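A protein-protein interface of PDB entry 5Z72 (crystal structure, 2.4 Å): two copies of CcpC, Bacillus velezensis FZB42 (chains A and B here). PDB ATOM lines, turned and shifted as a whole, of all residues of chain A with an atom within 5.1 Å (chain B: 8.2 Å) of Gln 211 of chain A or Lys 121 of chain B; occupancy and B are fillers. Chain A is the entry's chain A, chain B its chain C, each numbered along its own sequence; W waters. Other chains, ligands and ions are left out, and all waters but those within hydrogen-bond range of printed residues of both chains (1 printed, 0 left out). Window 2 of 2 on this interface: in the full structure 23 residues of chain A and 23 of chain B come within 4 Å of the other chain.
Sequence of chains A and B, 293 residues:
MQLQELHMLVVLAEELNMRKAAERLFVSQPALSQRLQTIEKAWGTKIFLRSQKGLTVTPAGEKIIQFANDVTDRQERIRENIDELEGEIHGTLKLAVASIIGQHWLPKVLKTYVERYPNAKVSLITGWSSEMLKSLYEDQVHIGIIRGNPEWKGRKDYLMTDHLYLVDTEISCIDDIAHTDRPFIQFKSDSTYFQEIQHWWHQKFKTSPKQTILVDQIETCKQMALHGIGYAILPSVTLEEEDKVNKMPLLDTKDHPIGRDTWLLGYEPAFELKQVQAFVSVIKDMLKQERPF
Of chain B, only Lys 121 (2.3 Å) comes within 4 Å of Gln 211 of chain A.
Of chain A, only Gln 211 and Thr 212 come within 4 Å of Lys 121 of chain B.
Of the printed residues of chain A, Leu 124 of chain B touches Leu 214.
Of the printed residues of chain A, Ser 123 of chain B touches Leu 214.
Tyr 117 of chain B touches none of the printed residues of chain A.
The nearest residue of chain B that does not touch Gln 211 of chain A is Val 122 of chain B (6.1 Å).
Hydrophobic or aromatic side chains of chain A within 4 Å of the printed part of chain B: Ile 213.
Of the 18 printed residues of chain B, 4 touch a printed residue of chain A.
Hydrophobic or aromatic side chains of chain B that line the printed part of chain A: Leu 124.
Among the printed residues, no Asp or Glu carboxylate lies within 4 Å of a Lys or Arg side-chain nitrogen of the other chain.
No position is printed for both chains.
Of the 7 pairs that touch across the chains among the printed residues, none has its exchanged pair printed and touching as well.
O of Thr 212 of chain A touches CA of Lys 121 of chain B, at 3.8 Å.
CA of Ile 213 of chain A touches O of Val 122 of chain B, at 3.3 Å.
CA of Ser 123 of chain B touches O of Leu 214 of chain A (3.5 Å).
NE2 of Gln 211 of chain A sits at hydrogen-bond distance from OE1 of Gln 186 of chain A (3.2 Å).
The backbone carbonyl oxygen (O) of Ile 213 of chain A is in hydrogen-bond range of the backbone NH (N) of Gln 186 of chain A, at 2.9 Å.
The backbone NH (N) of Leu 93 of chain B sits at hydrogen-bond distance from the backbone carbonyl oxygen (O) of Lys 121 of chain B, 2.9 Å away.
The backbone NH of Ser 123 of chain B lies within hydrogen-bond range of the backbone carbonyl oxygen of Leu 93 of chain B, at 2.9 Å.
The backbone carbonyl oxygen (O) of Ser 123 of chain B is in hydrogen-bond range of the backbone NH (N) of Leu 95 of chain B, at 2.9 Å.
Water W1 bridges O of Leu 124 of chain B (3.1 Å) and O of Leu 214 of chain A (3.1 Å).
O of Thr 212 of chain A lies within hydrogen-bond range of N of Val 122 of chain B (3.3 Å).
The backbone carbonyl oxygen of Val 122 of chain B is in hydrogen-bond range of the backbone NH of Leu 214 of chain A.
The backbone NH of Leu 124 of chain B lies within hydrogen-bond range of the backbone carbonyl oxygen of Leu 214 of chain A (2.8 Å).
NZ of Lys 121 of chain B sits close to O of Gln 211 of chain A (2.3 Å).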
ATOM      1  N   GLN A 186       7.250  15.668 -12.429  1.00  0.00           N
ATOM      2  CA  GLN A 186       5.839  15.596 -12.433  1.00  0.00           C
ATOM      3  C   GLN A 186       5.165  16.877 -12.905  1.00  0.00           C
ATOM      4  O   GLN A 186       5.404  17.976 -12.342  1.00  0.00           O
ATOM      5  CB  GLN A 186       5.456  15.267 -11.027  1.00  0.00           C
ATOM      6  CG  GLN A 186       4.058  15.379 -10.684  1.00  0.00           C
ATOM      7  CD  GLN A 186       3.765  14.381  -9.598  1.00  0.00           C
ATOM      8  OE1 GLN A 186       4.444  14.367  -8.568  1.00  0.00           O
ATOM      9  NE2 GLN A 186       2.790  13.510  -9.837  1.00  0.00           N
ATOM     10  N   PHE A 194      -2.751  15.481 -13.398  1.00  0.00           N
ATOM     11  CA  PHE A 194      -1.993  15.163 -12.223  1.00  0.00           C
ATOM     12  C   PHE A 194      -2.806  14.208 -11.322  1.00  0.00           C
ATOM     13  O   PHE A 194      -2.330  13.138 -10.927  1.00  0.00           O
ATOM     14  CB  PHE A 194      -1.597  16.487 -11.532  1.00  0.00           C
ATOM     15  CG  PHE A 194      -0.878  16.308 -10.240  1.00  0.00           C
ATOM     16  CD1 PHE A 194       0.488  16.207 -10.209  1.00  0.00           C
ATOM     17  CD2 PHE A 194      -1.592  16.224  -9.051  1.00  0.00           C
ATOM     18  CE1 PHE A 194       1.150  16.042  -9.015  1.00  0.00           C
ATOM     19  CE2 PHE A 194      -0.946  16.058  -7.867  1.00  0.00           C
ATOM     20  CZ  PHE A 194       0.439  15.975  -7.848  1.00  0.00           C
ATOM     21  N   GLN A 198      -1.774  10.420 -10.210  1.00  0.00           N
ATOM     22  CA  GLN A 198      -1.655  10.067  -8.794  1.00  0.00           C
ATOM     23  C   GLN A 198      -2.490   8.794  -8.507  1.00  0.00           C
ATOM     24  O   GLN A 198      -1.989   7.806  -7.935  1.00  0.00           O
ATOM     25  CB  GLN A 198      -2.119  11.218  -7.918  1.00  0.00           C
ATOM     26  CG  GLN A 198      -1.297  12.462  -8.050  1.00  0.00           C
ATOM     27  CD  GLN A 198      -0.039  12.353  -7.263  1.00  0.00           C
ATOM     28  OE1 GLN A 198       1.048  12.180  -7.825  1.00  0.00           O
ATOM     29  NE2 GLN A 198      -0.175  12.411  -5.937  1.00  0.00           N
ATOM     30  N   PRO A 209       3.922   8.568  -4.631  1.00  0.00           N
ATOM     31  CA  PRO A 209       5.101   8.955  -5.388  1.00  0.00           C
ATOM     32  C   PRO A 209       5.822  10.156  -4.726  1.00  0.00           C
ATOM     33  O   PRO A 209       5.211  10.996  -4.018  1.00  0.00           O
ATOM     34  CB  PRO A 209       4.516   9.318  -6.749  1.00  0.00           C
ATOM     35  CG  PRO A 209       3.085   9.801  -6.432  1.00  0.00           C
ATOM     36  CD  PRO A 209       2.761   9.392  -5.011  1.00  0.00           C
ATOM     37  N   LYS A 210       7.122  10.229  -4.986  1.00  0.00           N
ATOM     38  CA  LYS A 210       7.987  11.264  -4.407  1.00  0.00           C
ATOM     39  C   LYS A 210       7.909  12.657  -5.138  1.00  0.00           C
ATOM     40  O   LYS A 210       8.425  12.859  -6.237  1.00  0.00           O
ATOM     41  CB  LYS A 210       9.425  10.711  -4.362  1.00  0.00           C
ATOM     42  CG  LYS A 210       9.658   9.640  -3.270  1.00  0.00           C
ATOM     43  CD  LYS A 210       9.605   8.187  -3.816  1.00  0.00           C
ATOM     44  CE  LYS A 210      10.136   7.138  -2.802  1.00  0.00           C
ATOM     45  NZ  LYS A 210      10.438   5.774  -3.401  1.00  0.00           N
ATOM     46  N   GLN A 211       7.242  13.606  -4.482  1.00  0.00           N
ATOM     47  CA  GLN A 211       7.051  14.955  -4.992  1.00  0.00           C
ATOM     48  C   GLN A 211       8.368  15.767  -4.895  1.00  0.00           C
ATOM     49  O   GLN A 211       8.496  16.684  -4.059  1.00  0.00           O
ATOM     50  CB  GLN A 211       5.916  15.631  -4.196  1.00  0.00           C
ATOM     51  CG  GLN A 211       5.051  16.678  -4.941  1.00  0.00           C
ATOM     52  CD  GLN A 211       3.574  16.210  -5.186  1.00  0.00           C
ATOM     53  OE1 GLN A 211       2.620  16.979  -4.974  1.00  0.00           O
ATOM     54  NE2 GLN A 211       3.398  14.961  -5.642  1.00  0.00           N
ATOM     55  N   THR A 212       9.362  15.430  -5.723  1.00  0.00           N
ATOM     56  CA  THR A 212      10.564  16.249  -5.759  1.00  0.00           C
ATOM     57  C   THR A 212      10.393  17.360  -6.788  1.00  0.00           C
ATOM     58  O   THR A 212      10.170  18.525  -6.423  1.00  0.00           O
ATOM     59  CB  THR A 212      11.828  15.439  -6.053  1.00  0.00           C
ATOM     60  OG1 THR A 212      11.860  15.031  -7.426  1.00  0.00           O
ATOM     61  CG2 THR A 212      11.903  14.229  -5.116  1.00  0.00           C
ATOM     62  N   ILE A 213      10.458  17.012  -8.067  1.00  0.00           N
ATOM     63  CA  ILE A 213      10.308  18.015  -9.106  1.00  0.00           C
ATOM     64  C   ILE A 213       8.870  18.136  -9.633  1.00  0.00           C
ATOM     65  O   ILE A 213       8.278  17.202 -10.184  1.00  0.00           O
ATOM     66  CB  ILE A 213      11.250  17.747 -10.266  1.00  0.00           C
ATOM     67  CG1 ILE A 213      12.626  17.352  -9.726  1.00  0.00           C
ATOM     68  CG2 ILE A 213      11.321  18.976 -11.148  1.00  0.00           C
ATOM     69  CD1 ILE A 213      13.716  17.334 -10.758  1.00  0.00           C
ATOM     70  N   LEU A 214       8.376  19.350  -9.468  1.00  0.00           N
ATOM     71  CA  LEU A 214       7.080  19.784  -9.872  1.00  0.00           C
ATOM     72  C   LEU A 214       7.180  20.863 -10.971  1.00  0.00           C
ATOM     73  O   LEU A 214       7.744  21.935 -10.749  1.00  0.00           O
ATOM     74  CB  LEU A 214       6.356  20.317  -8.644  1.00  0.00           C
ATOM     75  CG  LEU A 214       4.840  20.410  -8.691  1.00  0.00           C
ATOM     76  CD1 LEU A 214       4.245  19.035  -8.926  1.00  0.00           C
ATOM     77  CD2 LEU A 214       4.329  21.005  -7.388  1.00  0.00           C
ATOM     78  N   GLY B  91      16.070  21.772   1.506  1.00  0.00           N
ATOM     79  CA  GLY B  91      15.081  22.824   1.287  1.00  0.00           C
ATOM     80  C   GLY B  91      14.645  22.903  -0.174  1.00  0.00           C
ATOM     81  O   GLY B  91      15.397  22.514  -1.081  1.00  0.00           O
ATOM     82  N   THR B  92      13.435  23.405  -0.411  1.00  0.00           N
ATOM     83  CA  THR B  92      12.828  23.302  -1.739  1.00  0.00           C
ATOM     84  C   THR B  92      12.958  24.578  -2.542  1.00  0.00           C
ATOM     85  O   THR B  92      12.542  25.653  -2.103  1.00  0.00           O
ATOM     86  CB  THR B  92      11.330  22.921  -1.651  1.00  0.00           C
ATOM     87  OG1 THR B  92      11.217  21.538  -1.273  1.00  0.00           O
ATOM     88  CG2 THR B  92      10.617  23.159  -2.997  1.00  0.00           C
ATOM     89  N   LEU B  93      13.524  24.446  -3.737  1.00  0.00           N
ATOM     90  CA  LEU B  93      13.838  25.610  -4.542  1.00  0.00           C
ATOM     91  C   LEU B  93      12.642  25.977  -5.398  1.00  0.00           C
ATOM     92  O   LEU B  93      12.182  25.178  -6.224  1.00  0.00           O
ATOM     93  CB  LEU B  93      15.062  25.317  -5.410  1.00  0.00           C
ATOM     94  CG  LEU B  93      15.448  26.347  -6.484  1.00  0.00           C
ATOM     95  CD1 LEU B  93      15.604  27.733  -5.915  1.00  0.00           C
ATOM     96  CD2 LEU B  93      16.712  25.894  -7.189  1.00  0.00           C
ATOM     97  N   LYS B  94      12.141  27.184  -5.223  1.00  0.00           N
ATOM     98  CA  LYS B  94      11.025  27.634  -6.008  1.00  0.00           C
ATOM     99  C   LYS B  94      11.379  28.624  -7.135  1.00  0.00           C
ATOM    100  O   LYS B  94      11.414  29.836  -6.889  1.00  0.00           O
ATOM    101  CB  LYS B  94      10.009  28.269  -5.070  1.00  0.00           C
ATOM    102  CG  LYS B  94       9.517  27.286  -4.029  1.00  0.00           C
ATOM    103  CD  LYS B  94       8.500  27.899  -3.093  1.00  0.00           C
ATOM    104  CE  LYS B  94       8.550  27.174  -1.752  1.00  0.00           C
ATOM    105  NZ  LYS B  94       7.533  27.699  -0.819  1.00  0.00           N
ATOM    106  N   LEU B  95      11.537  28.123  -8.369  1.00  0.00           N
ATOM    107  CA  LEU B  95      11.899  28.959  -9.526  1.00  0.00           C
ATOM    108  C   LEU B  95      10.762  29.494 -10.421  1.00  0.00           C
ATOM    109  O   LEU B  95       9.776  28.824 -10.712  1.00  0.00           O
ATOM    110  CB  LEU B  95      12.849  28.188 -10.437  1.00  0.00           C
ATOM    111  CG  LEU B  95      14.055  27.523  -9.789  1.00  0.00           C
ATOM    112  CD1 LEU B  95      14.647  26.527 -10.775  1.00  0.00           C
ATOM    113  CD2 LEU B  95      15.111  28.574  -9.304  1.00  0.00           C
ATOM    114  N   LEU B 110      19.593  22.158 -14.293  1.00  0.00           N
ATOM    115  CA  LEU B 110      18.897  21.338 -13.291  1.00  0.00           C
ATOM    116  C   LEU B 110      19.461  19.942 -13.265  1.00  0.00           C
ATOM    117  O   LEU B 110      19.553  19.323 -12.231  1.00  0.00           O
ATOM    118  CB  LEU B 110      17.391  21.276 -13.548  1.00  0.00           C
ATOM    119  CG  LEU B 110      16.560  22.239 -12.703  1.00  0.00           C
ATOM    120  CD1 LEU B 110      15.131  22.214 -13.211  1.00  0.00           C
ATOM    121  CD2 LEU B 110      16.622  21.899 -11.228  1.00  0.00           C
ATOM    122  N   TYR B 113      22.393  20.359 -11.070  1.00  0.00           N
ATOM    123  CA  TYR B 113      21.927  20.624  -9.724  1.00  0.00           C
ATOM    124  C   TYR B 113      21.356  19.393  -9.031  1.00  0.00           C
ATOM    125  O   TYR B 113      21.539  19.234  -7.835  1.00  0.00           O
ATOM    126  CB  TYR B 113      20.884  21.699  -9.755  1.00  0.00           C
ATOM    127  CG  TYR B 113      20.295  22.012  -8.419  1.00  0.00           C
ATOM    128  CD1 TYR B 113      20.984  22.789  -7.502  1.00  0.00           C
ATOM    129  CD2 TYR B 113      19.030  21.553  -8.069  1.00  0.00           C
ATOM    130  CE1 TYR B 113      20.422  23.109  -6.272  1.00  0.00           C
ATOM    131  CE2 TYR B 113      18.467  21.867  -6.850  1.00  0.00           C
ATOM    132  CZ  TYR B 113      19.160  22.641  -5.954  1.00  0.00           C
ATOM    133  OH  TYR B 113      18.613  22.956  -4.749  1.00  0.00           O
ATOM    134  N   VAL B 114      20.643  18.541  -9.773  1.00  0.00           N
ATOM    135  CA  VAL B 114      20.061  17.325  -9.209  1.00  0.00           C
ATOM    136  C   VAL B 114      21.191  16.336  -8.990  1.00  0.00           C
ATOM    137  O   VAL B 114      21.249  15.649  -7.987  1.00  0.00           O
ATOM    138  CB  VAL B 114      18.933  16.686 -10.146  1.00  0.00           C
ATOM    139  CG1 VAL B 114      18.576  15.301  -9.690  1.00  0.00           C
ATOM    140  CG2 VAL B 114      17.675  17.545 -10.164  1.00  0.00           C
ATOM    141  N   TYR B 117      23.033  17.212  -5.910  1.00  0.00           N
ATOM    142  CA  TYR B 117      22.203  17.360  -4.707  1.00  0.00           C
ATOM    143  C   TYR B 117      20.957  16.462  -4.742  1.00  0.00           C
ATOM    144  O   TYR B 117      19.817  16.952  -4.774  1.00  0.00           O
ATOM    145  CB  TYR B 117      21.776  18.802  -4.509  1.00  0.00           C
ATOM    146  CG  TYR B 117      22.914  19.773  -4.389  1.00  0.00           C
ATOM    147  CD1 TYR B 117      23.749  19.770  -3.285  1.00  0.00           C
ATOM    148  CD2 TYR B 117      23.135  20.726  -5.384  1.00  0.00           C
ATOM    149  CE1 TYR B 117      24.792  20.687  -3.184  1.00  0.00           C
ATOM    150  CE2 TYR B 117      24.163  21.632  -5.296  1.00  0.00           C
ATOM    151  CZ  TYR B 117      24.998  21.620  -4.197  1.00  0.00           C
ATOM    152  OH  TYR B 117      26.037  22.545  -4.132  1.00  0.00           O
ATOM    153  N   PRO B 118      21.185  15.138  -4.705  1.00  0.00           N
ATOM    154  CA  PRO B 118      20.122  14.141  -4.746  1.00  0.00           C
ATOM    155  C   PRO B 118      19.043  14.437  -3.730  1.00  0.00           C
ATOM    156  O   PRO B 118      19.351  14.868  -2.623  1.00  0.00           O
ATOM    157  CB  PRO B 118      20.852  12.844  -4.405  1.00  0.00           C
ATOM    158  CG  PRO B 118      22.252  13.060  -4.837  1.00  0.00           C
ATOM    159  CD  PRO B 118      22.518  14.511  -4.576  1.00  0.00           C
ATOM    160  N   ASN B 119      17.795  14.219  -4.123  1.00  0.00           N
ATOM    161  CA  ASN B 119      16.646  14.341  -3.222  1.00  0.00           C
ATOM    162  C   ASN B 119      16.312  15.785  -2.868  1.00  0.00           C
ATOM    163  O   ASN B 119      15.535  16.040  -1.946  1.00  0.00           O
ATOM    164  CB  ASN B 119      16.864  13.568  -1.913  1.00  0.00           C
ATOM    165  CG  ASN B 119      17.514  12.218  -2.120  1.00  0.00           C
ATOM    166  OD1 ASN B 119      17.338  11.564  -3.163  1.00  0.00           O
ATOM    167  ND2 ASN B 119      18.279  11.786  -1.111  1.00  0.00           N
ATOM    168  N   ALA B 120      16.892  16.727  -3.590  1.00  0.00           N
ATOM    169  CA  ALA B 120      16.561  18.122  -3.364  1.00  0.00           C
ATOM    170  C   ALA B 120      15.376  18.517  -4.246  1.00  0.00           C
ATOM    171  O   ALA B 120      15.317  18.227  -5.441  1.00  0.00           O
ATOM    172  CB  ALA B 120      17.752  18.991  -3.629  1.00  0.00           C
ATOM    173  N   LYS B 121      14.424  19.184  -3.632  1.00  0.00           N
ATOM    174  CA  LYS B 121      13.189  19.461  -4.284  1.00  0.00           C
ATOM    175  C   LYS B 121      13.236  20.735  -5.112  1.00  0.00           C
ATOM    176  O   LYS B 121      13.811  21.737  -4.700  1.00  0.00           O
ATOM    177  CB  LYS B 121      12.095  19.545  -3.223  1.00  0.00           C
ATOM    178  CG  LYS B 121      11.724  18.199  -2.591  1.00  0.00           C
ATOM    179  CD  LYS B 121      10.673  18.387  -1.506  1.00  0.00           C
ATOM    180  CE  LYS B 121      10.157  17.073  -0.957  1.00  0.00           C
ATOM    181  NZ  LYS B 121       9.240  16.414  -1.948  1.00  0.00           N
ATOM    182  N   VAL B 122      12.581  20.707  -6.267  1.00  0.00           N
ATOM    183  CA  VAL B 122      12.477  21.879  -7.126  1.00  0.00           C
ATOM    184  C   VAL B 122      11.051  22.066  -7.621  1.00  0.00           C
ATOM    185  O   VAL B 122      10.487  21.170  -8.214  1.00  0.00           O
ATOM    186  CB  VAL B 122      13.388  21.758  -8.370  1.00  0.00           C
ATOM    187  CG1 VAL B 122      13.452  23.055  -9.061  1.00  0.00           C
ATOM    188  CG2 VAL B 122      14.777  21.302  -7.991  1.00  0.00           C
ATOM    189  N   SER B 123      10.480  23.229  -7.427  1.00  0.00           N
ATOM    190  CA  SER B 123       9.234  23.536  -8.056  1.00  0.00           C
ATOM    191  C   SER B 123       9.434  24.663  -9.101  1.00  0.00           C
ATOM    192  O   SER B 123      10.085  25.711  -8.839  1.00  0.00           O
ATOM    193  CB  SER B 123       8.204  23.911  -7.000  1.00  0.00           C
ATOM    194  OG  SER B 123       7.961  25.304  -7.010  1.00  0.00           O
ATOM    195  N   LEU B 124       8.854  24.453 -10.286  1.00  0.00           N
ATOM    196  CA  LEU B 124       9.141  25.339 -11.405  1.00  0.00           C
ATOM    197  C   LEU B 124       7.913  25.881 -12.088  1.00  0.00           C
ATOM    198  O   LEU B 124       7.125  25.126 -12.633  1.00  0.00           O
ATOM    199  CB  LEU B 124      10.027  24.605 -12.418  1.00  0.00           C
ATOM    200  CG  LEU B 124      10.320  25.297 -13.752  1.00  0.00           C
ATOM    201  CD1 LEU B 124      11.096  26.598 -13.555  1.00  0.00           C
ATOM    202  CD2 LEU B 124      11.061  24.343 -14.692  1.00  0.00           C
ATOM    203  N   HIS B 142      11.497  31.925  -4.849  1.00  0.00           N
ATOM    204  CA  HIS B 142      12.849  32.389  -4.511  1.00  0.00           C
ATOM    205  C   HIS B 142      13.559  33.217  -5.601  1.00  0.00           C
ATOM    206  O   HIS B 142      13.928  34.351  -5.371  1.00  0.00           O
ATOM    207  CB  HIS B 142      13.713  31.185  -4.181  1.00  0.00           C
ATOM    208  CG  HIS B 142      13.193  30.415  -3.030  1.00  0.00           C
ATOM    209  ND1 HIS B 142      13.513  29.094  -2.802  1.00  0.00           N
ATOM    210  CD2 HIS B 142      12.343  30.780  -2.040  1.00  0.00           C
ATOM    211  CE1 HIS B 142      12.886  28.680  -1.713  1.00  0.00           C
ATOM    212  NE2 HIS B 142      12.175  29.685  -1.230  1.00  0.00           N
ATOM    213  N   GLN B 275      19.668  26.202  -0.601  1.00  0.00           N
ATOM    214  CA  GLN B 275      19.486  25.590  -1.902  1.00  0.00           C
ATOM    215  C   GLN B 275      19.519  26.675  -2.985  1.00  0.00           C
ATOM    216  O   GLN B 275      19.975  26.419  -4.096  1.00  0.00           O
ATOM    217  CB  GLN B 275      18.175  24.789  -1.963  1.00  0.00           C
ATOM    218  CG  GLN B 275      16.892  25.616  -1.940  1.00  0.00           C
ATOM    219  CD  GLN B 275      16.546  26.160  -0.565  1.00  0.00           C
ATOM    220  OE1 GLN B 275      17.381  26.181   0.352  1.00  0.00           O
ATOM    221  NE2 GLN B 275      15.307  26.622  -0.419  1.00  0.00           N
HETATM  222  O   HOH W   1       5.274  23.822 -10.504  1.00  0.00           O
